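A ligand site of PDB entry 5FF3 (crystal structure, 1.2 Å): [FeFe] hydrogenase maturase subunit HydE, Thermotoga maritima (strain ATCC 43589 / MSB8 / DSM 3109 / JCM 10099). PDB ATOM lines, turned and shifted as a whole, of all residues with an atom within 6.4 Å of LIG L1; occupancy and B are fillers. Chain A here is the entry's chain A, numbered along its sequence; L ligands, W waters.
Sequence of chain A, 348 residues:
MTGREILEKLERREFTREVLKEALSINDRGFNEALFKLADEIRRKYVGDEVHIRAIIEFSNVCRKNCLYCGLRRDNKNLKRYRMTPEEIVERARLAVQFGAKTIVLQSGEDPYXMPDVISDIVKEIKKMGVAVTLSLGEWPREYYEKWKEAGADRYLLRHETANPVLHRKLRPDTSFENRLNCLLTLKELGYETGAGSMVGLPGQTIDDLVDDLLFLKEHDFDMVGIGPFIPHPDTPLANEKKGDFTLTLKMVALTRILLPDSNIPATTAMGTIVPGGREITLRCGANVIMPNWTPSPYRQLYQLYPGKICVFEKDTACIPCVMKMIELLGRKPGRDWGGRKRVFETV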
ATOM      1  N   VAL A  62      11.204  10.079 -26.649  1.00  0.00           N
ATOM      2  CA  VAL A  62      11.594   9.200 -27.790  1.00  0.00           C
ATOM      3  C   VAL A  62      10.482   8.195 -27.984  1.00  0.00           C
ATOM      4  O   VAL A  62      10.025   7.559 -27.023  1.00  0.00           O
ATOM      5  CB  VAL A  62      12.945   8.566 -27.522  1.00  0.00           C
ATOM      6  CG1 VAL A  62      13.307   7.508 -28.558  1.00  0.00           C
ATOM      7  CG2 VAL A  62      14.024   9.660 -27.412  1.00  0.00           C
ATOM      8  N   CYS A  63      10.075   7.998 -29.248  1.00  0.00           N
ATOM      9  CA  CYS A  63       9.134   6.942 -29.520  1.00  0.00           C
ATOM     10  C   CYS A  63       9.459   6.239 -30.854  1.00  0.00           C
ATOM     11  O   CYS A  63       9.757   6.863 -31.865  1.00  0.00           O
ATOM     12  CB  CYS A  63       7.690   7.447 -29.558  1.00  0.00           C
ATOM     13  SG  CYS A  63       6.486   6.062 -29.452  1.00  0.00           S
ATOM     14  N   ARG A  64       9.278   4.908 -30.804  1.00  0.00           N
ATOM     15  CA  ARG A  64       9.376   4.049 -31.988  1.00  0.00           C
ATOM     16  C   ARG A  64       8.115   3.912 -32.799  1.00  0.00           C
ATOM     17  O   ARG A  64       8.181   3.422 -33.971  1.00  0.00           O
ATOM     18  CB  ARG A  64       9.854   2.632 -31.583  1.00  0.00           C
ATOM     19  CG  ARG A  64       8.785   1.848 -30.807  1.00  0.00           C
ATOM     20  CD  ARG A  64       9.293   0.549 -30.282  1.00  0.00           C
ATOM     21  NE  ARG A  64       8.302  -0.108 -29.491  1.00  0.00           N
ATOM     22  CZ  ARG A  64       8.330  -1.367 -29.125  1.00  0.00           C
ATOM     23  NH1 ARG A  64       9.300  -2.162 -29.510  1.00  0.00           N
ATOM     24  NH2 ARG A  64       7.302  -1.871 -28.425  1.00  0.00           N
ATOM     25  N   LYS A  65       6.968   4.317 -32.245  1.00  0.00           N
ATOM     26  CA  LYS A  65       5.712   4.191 -32.937  1.00  0.00           C
ATOM     27  C   LYS A  65       5.372   5.484 -33.660  1.00  0.00           C
ATOM     28  O   LYS A  65       6.001   6.507 -33.508  1.00  0.00           O
ATOM     29  CB  LYS A  65       4.584   3.765 -31.990  1.00  0.00           C
ATOM     30  CG  LYS A  65       4.585   2.264 -31.679  1.00  0.00           C
ATOM     31  CD  LYS A  65       3.407   1.818 -30.872  1.00  0.00           C
ATOM     32  CE  LYS A  65       3.187   0.318 -30.816  1.00  0.00           C
ATOM     33  NZ  LYS A  65       4.365  -0.476 -30.444  1.00  0.00           N
ATOM     34  N   ASN A  66       4.305   5.425 -34.487  1.00  0.00           N
ATOM     35  CA  ASN A  66       3.966   6.495 -35.412  1.00  0.00           C
ATOM     36  C   ASN A  66       2.496   6.836 -35.370  1.00  0.00           C
ATOM     37  O   ASN A  66       1.869   7.165 -36.411  1.00  0.00           O
ATOM     38  CB  ASN A  66       4.387   6.132 -36.859  1.00  0.00           C
ATOM     39  CG  ASN A  66       4.808   7.300 -37.669  1.00  0.00           C
ATOM     40  OD1 ASN A  66       5.227   8.323 -37.198  1.00  0.00           O
ATOM     41  ND2 ASN A  66       4.742   7.118 -39.020  1.00  0.00           N
ATOM     42  N   CYS A  67       1.906   6.767 -34.182  1.00  0.00           N
ATOM     43  CA  CYS A  67       0.459   7.040 -34.054  1.00  0.00           C
ATOM     44  C   CYS A  67       0.074   8.373 -34.687  1.00  0.00           C
ATOM     45  O   CYS A  67       0.789   9.366 -34.529  1.00  0.00           O
ATOM     46  CB  CYS A  67       0.030   7.016 -32.559  1.00  0.00           C
ATOM     47  SG  CYS A  67       0.534   5.500 -31.677  1.00  0.00           S
ATOM     48  N   LEU A  68      -1.029   8.388 -35.471  1.00  0.00           N
ATOM     49  CA  LEU A  68      -1.306   9.552 -36.327  1.00  0.00           C
ATOM     50  C   LEU A  68      -1.632  10.813 -35.597  1.00  0.00           C
ATOM     51  O   LEU A  68      -1.464  11.918 -36.092  1.00  0.00           O
ATOM     52  CB  LEU A  68      -2.423   9.203 -37.315  1.00  0.00           C
ATOM     53  CG  LEU A  68      -1.922   8.581 -38.642  1.00  0.00           C
ATOM     54  CD1 LEU A  68      -1.230   7.260 -38.483  1.00  0.00           C
ATOM     55  CD2 LEU A  68      -3.135   8.450 -39.582  1.00  0.00           C
ATOM     56  N   TYR A  69      -2.141  10.638 -34.363  1.00  0.00           N
ATOM     57  CA  TYR A  69      -2.611  11.747 -33.508  1.00  0.00           C
ATOM     58  C   TYR A  69      -1.530  12.386 -32.683  1.00  0.00           C
ATOM     59  O   TYR A  69      -1.726  13.508 -32.136  1.00  0.00           O
ATOM     60  CB  TYR A  69      -3.768  11.299 -32.581  1.00  0.00           C
ATOM     61  CG  TYR A  69      -3.529   9.992 -31.913  1.00  0.00           C
ATOM     62  CD1 TYR A  69      -2.746   9.897 -30.764  1.00  0.00           C
ATOM     63  CD2 TYR A  69      -4.081   8.761 -32.373  1.00  0.00           C
ATOM     64  CE1 TYR A  69      -2.495   8.701 -30.157  1.00  0.00           C
ATOM     65  CE2 TYR A  69      -3.853   7.579 -31.761  1.00  0.00           C
ATOM     66  CZ  TYR A  69      -3.050   7.525 -30.637  1.00  0.00           C
ATOM     67  OH  TYR A  69      -2.832   6.307 -30.069  1.00  0.00           O
ATOM     68  N   CYS A  70      -0.371  11.718 -32.503  1.00  0.00           N
ATOM     69  CA  CYS A  70       0.516  12.022 -31.387  1.00  0.00           C
ATOM     70  C   CYS A  70       1.699  12.846 -31.831  1.00  0.00           C
ATOM     71  O   CYS A  70       2.441  12.434 -32.785  1.00  0.00           O
ATOM     72  CB  CYS A  70       1.027  10.754 -30.798  1.00  0.00           C
ATOM     73  SG  CYS A  70       2.065  11.022 -29.316  1.00  0.00           S
ATOM     74  N   GLY A  71       2.020  13.945 -31.161  1.00  0.00           N
ATOM     75  CA  GLY A  71       3.158  14.742 -31.471  1.00  0.00           C
ATOM     76  C   GLY A  71       4.501  14.084 -31.271  1.00  0.00           C
ATOM     77  O   GLY A  71       5.539  14.541 -31.780  1.00  0.00           O
ATOM     78  N   LEU A  72       4.553  12.986 -30.486  1.00  0.00           N
ATOM     79  CA  LEU A  72       5.794  12.232 -30.271  1.00  0.00           C
ATOM     80  C   LEU A  72       6.042  11.162 -31.346  1.00  0.00           C
ATOM     81  O   LEU A  72       7.071  10.518 -31.322  1.00  0.00           O
ATOM     82  CB  LEU A  72       5.818  11.532 -28.892  1.00  0.00           C
ATOM     83  CG  LEU A  72       5.737  12.517 -27.729  1.00  0.00           C
ATOM     84  CD1 LEU A  72       6.066  11.682 -26.469  1.00  0.00           C
ATOM     85  CD2 LEU A  72       6.249  13.849 -27.706  1.00  0.00           C
ATOM     86  N   ARG A  73       5.133  11.049 -32.325  1.00  0.00           N
ATOM     87  CA  ARG A  73       5.269  10.012 -33.352  1.00  0.00           C
ATOM     88  C   ARG A  73       6.671  10.113 -33.992  1.00  0.00           C
ATOM     89  O   ARG A  73       7.240  11.165 -34.173  1.00  0.00           O
ATOM     90  CB  ARG A  73       4.145  10.143 -34.405  1.00  0.00           C
ATOM     91  CG  ARG A  73       4.206  11.433 -35.242  1.00  0.00           C
ATOM     92  CD  ARG A  73       2.899  11.685 -35.911  1.00  0.00           C
ATOM     93  NE  ARG A  73       2.413  10.545 -36.646  1.00  0.00           N
ATOM     94  CZ  ARG A  73       2.702  10.276 -37.975  1.00  0.00           C
ATOM     95  NH1 ARG A  73       3.402  11.109 -38.665  1.00  0.00           N
ATOM     96  NH2 ARG A  73       2.196   9.169 -38.471  1.00  0.00           N
ATOM     97  N   ARG A  74       7.180   8.905 -34.386  1.00  0.00           N
ATOM     98  CA  ARG A  74       8.567   8.851 -34.860  1.00  0.00           C
ATOM     99  C   ARG A  74       8.838   9.728 -36.078  1.00  0.00           C
ATOM    100  O   ARG A  74       9.941  10.229 -36.216  1.00  0.00           O
ATOM    101  CB  ARG A  74       9.018   7.459 -35.121  1.00  0.00           C
ATOM    102  CG  ARG A  74       8.427   6.750 -36.240  1.00  0.00           C
ATOM    103  CD  ARG A  74       9.153   5.405 -36.552  1.00  0.00           C
ATOM    104  NE  ARG A  74       8.465   4.881 -37.710  1.00  0.00           N
ATOM    105  CZ  ARG A  74       7.415   4.103 -37.703  1.00  0.00           C
ATOM    106  NH1 ARG A  74       7.013   3.515 -36.585  1.00  0.00           N
ATOM    107  NH2 ARG A  74       6.731   3.799 -38.835  1.00  0.00           N
ATOM    108  N   SER A 108       6.373   7.644 -20.778  1.00  0.00           N
ATOM    109  CA  SER A 108       7.298   7.993 -21.845  1.00  0.00           C
ATOM    110  C   SER A 108       6.687   7.571 -23.192  1.00  0.00           C
ATOM    111  O   SER A 108       5.708   6.829 -23.272  1.00  0.00           O
ATOM    112  CB  SER A 108       8.622   7.235 -21.666  1.00  0.00           C
ATOM    113  OG  SER A 108       8.461   5.829 -21.685  1.00  0.00           O
ATOM    114  N   GLY A 109       7.322   8.083 -24.260  1.00  0.00           N
ATOM    115  CA  GLY A 109       7.152   7.397 -25.542  1.00  0.00           C
ATOM    116  C   GLY A 109       7.647   5.981 -25.406  1.00  0.00           C
ATOM    117  O   GLY A 109       8.305   5.577 -24.425  1.00  0.00           O
ATOM    118  N   GLU A 110       7.390   5.195 -26.444  1.00  0.00           N
ATOM    119  CA  GLU A 110       7.932   3.818 -26.491  1.00  0.00           C
ATOM    120  C   GLU A 110       9.409   3.901 -26.865  1.00  0.00           C
ATOM    121  O   GLU A 110       9.791   3.735 -28.062  1.00  0.00           O
ATOM    122  CB  GLU A 110       7.158   2.923 -27.448  1.00  0.00           C
ATOM    123  CG  GLU A 110       5.775   2.583 -26.930  1.00  0.00           C
ATOM    124  CD  GLU A 110       5.116   1.411 -27.686  1.00  0.00           C
ATOM    125  OE1 GLU A 110       5.794   0.786 -28.524  1.00  0.00           O
ATOM    126  OE2 GLU A 110       3.926   1.158 -27.443  1.00  0.00           O
ATOM    127  N   GLY A 138       3.609   2.132 -22.755  1.00  0.00           N
ATOM    128  CA  GLY A 138       3.157   1.539 -24.027  1.00  0.00           C
ATOM    129  C   GLY A 138       3.178   0.023 -24.034  1.00  0.00           C
ATOM    130  O   GLY A 138       3.068  -0.633 -22.985  1.00  0.00           O
ATOM    131  N   GLU A 161      -7.593   3.571 -26.316  1.00  0.00           N
ATOM    132  CA  GLU A 161      -7.631   4.600 -27.344  1.00  0.00           C
ATOM    133  C   GLU A 161      -8.970   4.708 -28.106  1.00  0.00           C
ATOM    134  O   GLU A 161      -9.584   5.765 -28.133  1.00  0.00           O
ATOM    135  CB  GLU A 161      -6.450   4.492 -28.340  1.00  0.00           C
ATOM    136  CG  GLU A 161      -5.083   4.330 -27.668  1.00  0.00           C
ATOM    137  CD  GLU A 161      -4.624   5.479 -26.763  1.00  0.00           C
ATOM    138  OE1 GLU A 161      -5.401   6.425 -26.541  1.00  0.00           O
ATOM    139  OE2 GLU A 161      -3.481   5.363 -26.299  1.00  0.00           O
ATOM    140  N   ARG A 172      -3.147   3.848 -35.520  1.00  0.00           N
ATOM    141  CA  ARG A 172      -1.972   3.261 -34.818  1.00  0.00           C
ATOM    142  C   ARG A 172      -1.361   2.162 -35.690  1.00  0.00           C
ATOM    143  O   ARG A 172      -1.534   0.975 -35.438  1.00  0.00           O
ATOM    144  CB  ARG A 172      -2.399   2.793 -33.433  1.00  0.00           C
ATOM    145  CG  ARG A 172      -3.183   3.849 -32.685  1.00  0.00           C
ATOM    146  CD  ARG A 172      -3.439   3.457 -31.231  1.00  0.00           C
ATOM    147  NE  ARG A 172      -2.165   3.443 -30.490  1.00  0.00           N
ATOM    148  CZ  ARG A 172      -1.550   2.371 -30.024  1.00  0.00           C
ATOM    149  NH1 ARG A 172      -2.090   1.212 -29.992  1.00  0.00           N
ATOM    150  NH2 ARG A 172      -0.282   2.512 -29.594  1.00  0.00           N
ATOM    151  N   ARG A 180      -3.372  -4.325 -28.324  1.00  0.00           N
ATOM    152  CA  ARG A 180      -3.612  -3.442 -27.178  1.00  0.00           C
ATOM    153  C   ARG A 180      -4.380  -4.148 -26.076  1.00  0.00           C
ATOM    154  O   ARG A 180      -4.034  -4.088 -24.903  1.00  0.00           O
ATOM    155  CB  ARG A 180      -4.326  -2.199 -27.659  1.00  0.00           C
ATOM    156  CG  ARG A 180      -4.310  -0.985 -26.689  1.00  0.00           C
ATOM    157  CD  ARG A 180      -2.990  -0.319 -26.806  1.00  0.00           C
ATOM    158  NE  ARG A 180      -2.959   0.980 -26.126  1.00  0.00           N
ATOM    159  CZ  ARG A 180      -1.887   1.756 -26.014  1.00  0.00           C
ATOM    160  NH1 ARG A 180      -0.707   1.365 -26.541  1.00  0.00           N
ATOM    161  NH2 ARG A 180      -1.919   2.879 -25.333  1.00  0.00           N
ATOM    162  N   TYR A 303       7.596  17.579 -24.122  1.00  0.00           N
ATOM    163  CA  TYR A 303       6.724  16.416 -24.061  1.00  0.00           C
ATOM    164  C   TYR A 303       5.372  16.801 -24.505  1.00  0.00           C
ATOM    165  O   TYR A 303       4.516  17.175 -23.691  1.00  0.00           O
ATOM    166  CB  TYR A 303       6.727  15.788 -22.678  1.00  0.00           C
ATOM    167  CG  TYR A 303       6.083  14.405 -22.650  1.00  0.00           C
ATOM    168  CD1 TYR A 303       6.859  13.244 -22.935  1.00  0.00           C
ATOM    169  CD2 TYR A 303       4.748  14.243 -22.362  1.00  0.00           C
ATOM    170  CE1 TYR A 303       6.316  11.993 -22.886  1.00  0.00           C
ATOM    171  CE2 TYR A 303       4.204  13.008 -22.290  1.00  0.00           C
ATOM    172  CZ  TYR A 303       4.964  11.882 -22.590  1.00  0.00           C
ATOM    173  OH  TYR A 303       4.415  10.585 -22.478  1.00  0.00           O
ATOM    174  N   LEU A 305       2.466  15.595 -26.563  1.00  0.00           N
ATOM    175  CA  LEU A 305       1.530  14.690 -27.226  1.00  0.00           C
ATOM    176  C   LEU A 305       0.612  15.520 -28.047  1.00  0.00           C
ATOM    177  O   LEU A 305       0.250  15.157 -29.185  1.00  0.00           O
ATOM    178  CB  LEU A 305       0.749  13.906 -26.142  1.00  0.00           C
ATOM    179  CG  LEU A 305       1.604  13.094 -25.141  1.00  0.00           C
ATOM    180  CD1 LEU A 305       0.690  12.606 -24.018  1.00  0.00           C
ATOM    181  CD2 LEU A 305       2.302  11.944 -25.849  1.00  0.00           C
HETATM  182 FE1  LIG L   1       2.566   8.830 -28.941  1.00  0.00          FE
HETATM  183 FE2  LIG L   1       4.382   6.864 -29.156  1.00  0.00          FE
HETATM  184 FE3  LIG L   1       1.821   6.410 -29.948  1.00  0.00          FE
HETATM  185 FE4  LIG L   1       2.352   6.642 -27.110  1.00  0.00          FE
HETATM  186  S1  LIG L   1       3.076   4.995 -28.726  1.00  0.00           S
HETATM  187  S2  LIG L   1       0.647   7.676 -28.410  1.00  0.00           S
HETATM  188  S3  LIG L   1       4.090   8.301 -27.410  1.00  0.00           S
HETATM  189  S4  LIG L   1       3.340   7.852 -30.910  1.00  0.00           S
HETATM  190  N1  LG2 L   2       3.328   5.863 -25.334  1.00  0.00           N
HETATM  191  C1  LG2 L   2       2.436   5.501 -24.240  1.00  0.00           C
HETATM  192  C2  LG2 L   2       2.331   6.658 -23.198  1.00  0.00           C
HETATM  193  C3  LG2 L   2       2.245   8.090 -23.662  1.00  0.00           C
HETATM  194  S1  LG2 L   2       0.965   8.526 -24.784  1.00  0.00           S
HETATM  195  C4  LG2 L   2       1.158   5.064 -24.800  1.00  0.00           C
HETATM  196  O1  LG2 L   2       0.401   4.412 -24.052  1.00  0.00           O
HETATM  197  O2  LG2 L   2       0.926   5.303 -26.017  1.00  0.00           O
HETATM  198  C5  LG2 L   2      -0.359   8.744 -23.487  1.00  0.00           C
HETATM  199  C6  LG2 L   2      -1.802   9.037 -23.986  1.00  0.00           C
HETATM  200  O3  LG2 L   2      -1.914  10.388 -24.542  1.00  0.00           O
HETATM  201  C7  LG2 L   2      -2.319   8.208 -25.049  1.00  0.00           C
HETATM  202  O4  LG2 L   2      -2.800   6.980 -24.490  1.00  0.00           O
HETATM  203  C8  LG2 L   2      -3.392   9.024 -25.801  1.00  0.00           C
HETATM  204  O5  LG2 L   2      -4.728   8.749 -25.365  1.00  0.00           O
HETATM  205  C9  LG2 L   2      -3.080  10.457 -25.406  1.00  0.00           C
HETATM  206  N2  LG2 L   2      -2.732  11.361 -26.461  1.00  0.00           N
HETATM  207  C10 LG2 L   2      -1.787  11.176 -27.410  1.00  0.00           C
HETATM  208  N3  LG2 L   2      -1.827  12.081 -28.366  1.00  0.00           N
HETATM  209  C11 LG2 L   2      -2.902  12.869 -28.064  1.00  0.00           C
HETATM  210  C12 LG2 L   2      -3.519  13.997 -28.677  1.00  0.00           C
HETATM  211  N4  LG2 L   2      -3.144  14.490 -29.862  1.00  0.00           N
HETATM  212  N5  LG2 L   2      -4.613  14.531 -28.077  1.00  0.00           N
HETATM  213  C13 LG2 L   2      -5.074  14.061 -26.886  1.00  0.00           C
HETATM  214  N6  LG2 L   2      -4.536  13.049 -26.268  1.00  0.00           N
HETATM  215  C14 LG2 L   2      -3.487  12.427 -26.821  1.00  0.00           C
HETATM  216  O   HOH W   1      -1.395   5.213 -28.094  1.00  0.00           O
HETATM  217  O   HOH W   2       1.705   2.623 -26.965  1.00  0.00           O
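Water W1 lies within hydrogen-bond range of the side-chain hydroxyl (OH) of Tyr 69 (2.7 Å), the side-chain carboxylate (OE2) of Glu 161 (2.8 Å), the guanidinium group (NE) of Arg 172 (3.1 Å) and a sulfur (S2) of LIG L1 (3.2 Å). Water W2 lies within hydrogen-bond range of OE2 of Glu 110 (2.7 Å), NH1 of Arg 180 (2.8 Å), S1 of LIG L1 (3.3 Å) and NH2 of Arg 172 (3.3 Å).
Merely in contact with LIG L1: Lys 65 (3.8 Å), Tyr 69 (3.7 Å), Leu 72 (3.95 Å), Arg 73 (3.8 Å) and Gly 109 (3.7 Å). Of the 22 residues printed, 8 come within 4 Å of LIG L1.
An iron atom (FE2) of LIG L1 is bound by the side-chain sulfur (SG) of Cys 63. The side-chain sulfur (SG) of Cys 70 is bound to an iron atom (FE1) of LIG L1, 2.3 Å away. The backbone NH (N) of Cys 67 lies close to a sulfur (S4) of LIG L1 (3.7 Å). SG of Cys 67 is bound to FE3 of LIG L1 (2.3 Å). O of Tyr 69 sits at hydrogen-bond distance from N4 of LG2 L2 (2.9 Å). N1 of LG2 L2 sits close to O of Ser 108. The side-chain carboxylate (OE2) of Glu 161 lies within hydrogen-bond range of an oxygen (O4) of LG2 L2 (2.5 Å). The guanidinium group (NH2) of Arg 180 lies within salt-bridge range of an oxygen (O1) of LG2 L2 (3.1 Å).
N of Lys 65 sits close to SG of Cys 63 (3.3 Å). The side-chain sulfur (SG) of Cys 63 lies close to the backbone NH (N) of Glu 110, 3.3 Å away. The side-chain sulfur of Cys 70 lies close to the backbone NH of Leu 72, 3.4 Å away. The side-chain sulfur (SG) of Cys 67 lies close to the guanidinium group (NE) of Arg 172. The side-chain hydroxyl of Tyr 69 is in hydrogen-bond range of the guanidinium group of Arg 172 (3.0 Å). The guanidinium group of Arg 73 sits at hydrogen-bond distance from the backbone carbonyl oxygen of Asn 66, at 2.9 Å. OE1 of Glu 110 is in salt-bridge range of NZ of Lys 65 (2.7 Å). The backbone carbonyl oxygen of Lys 65 is in hydrogen-bond range of the backbone NH of Arg 74 (2.8 Å).
A nitrogen (N1) of LG2 L2 is bound to an iron atom (FE4) of LIG L1 (2.2 Å).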
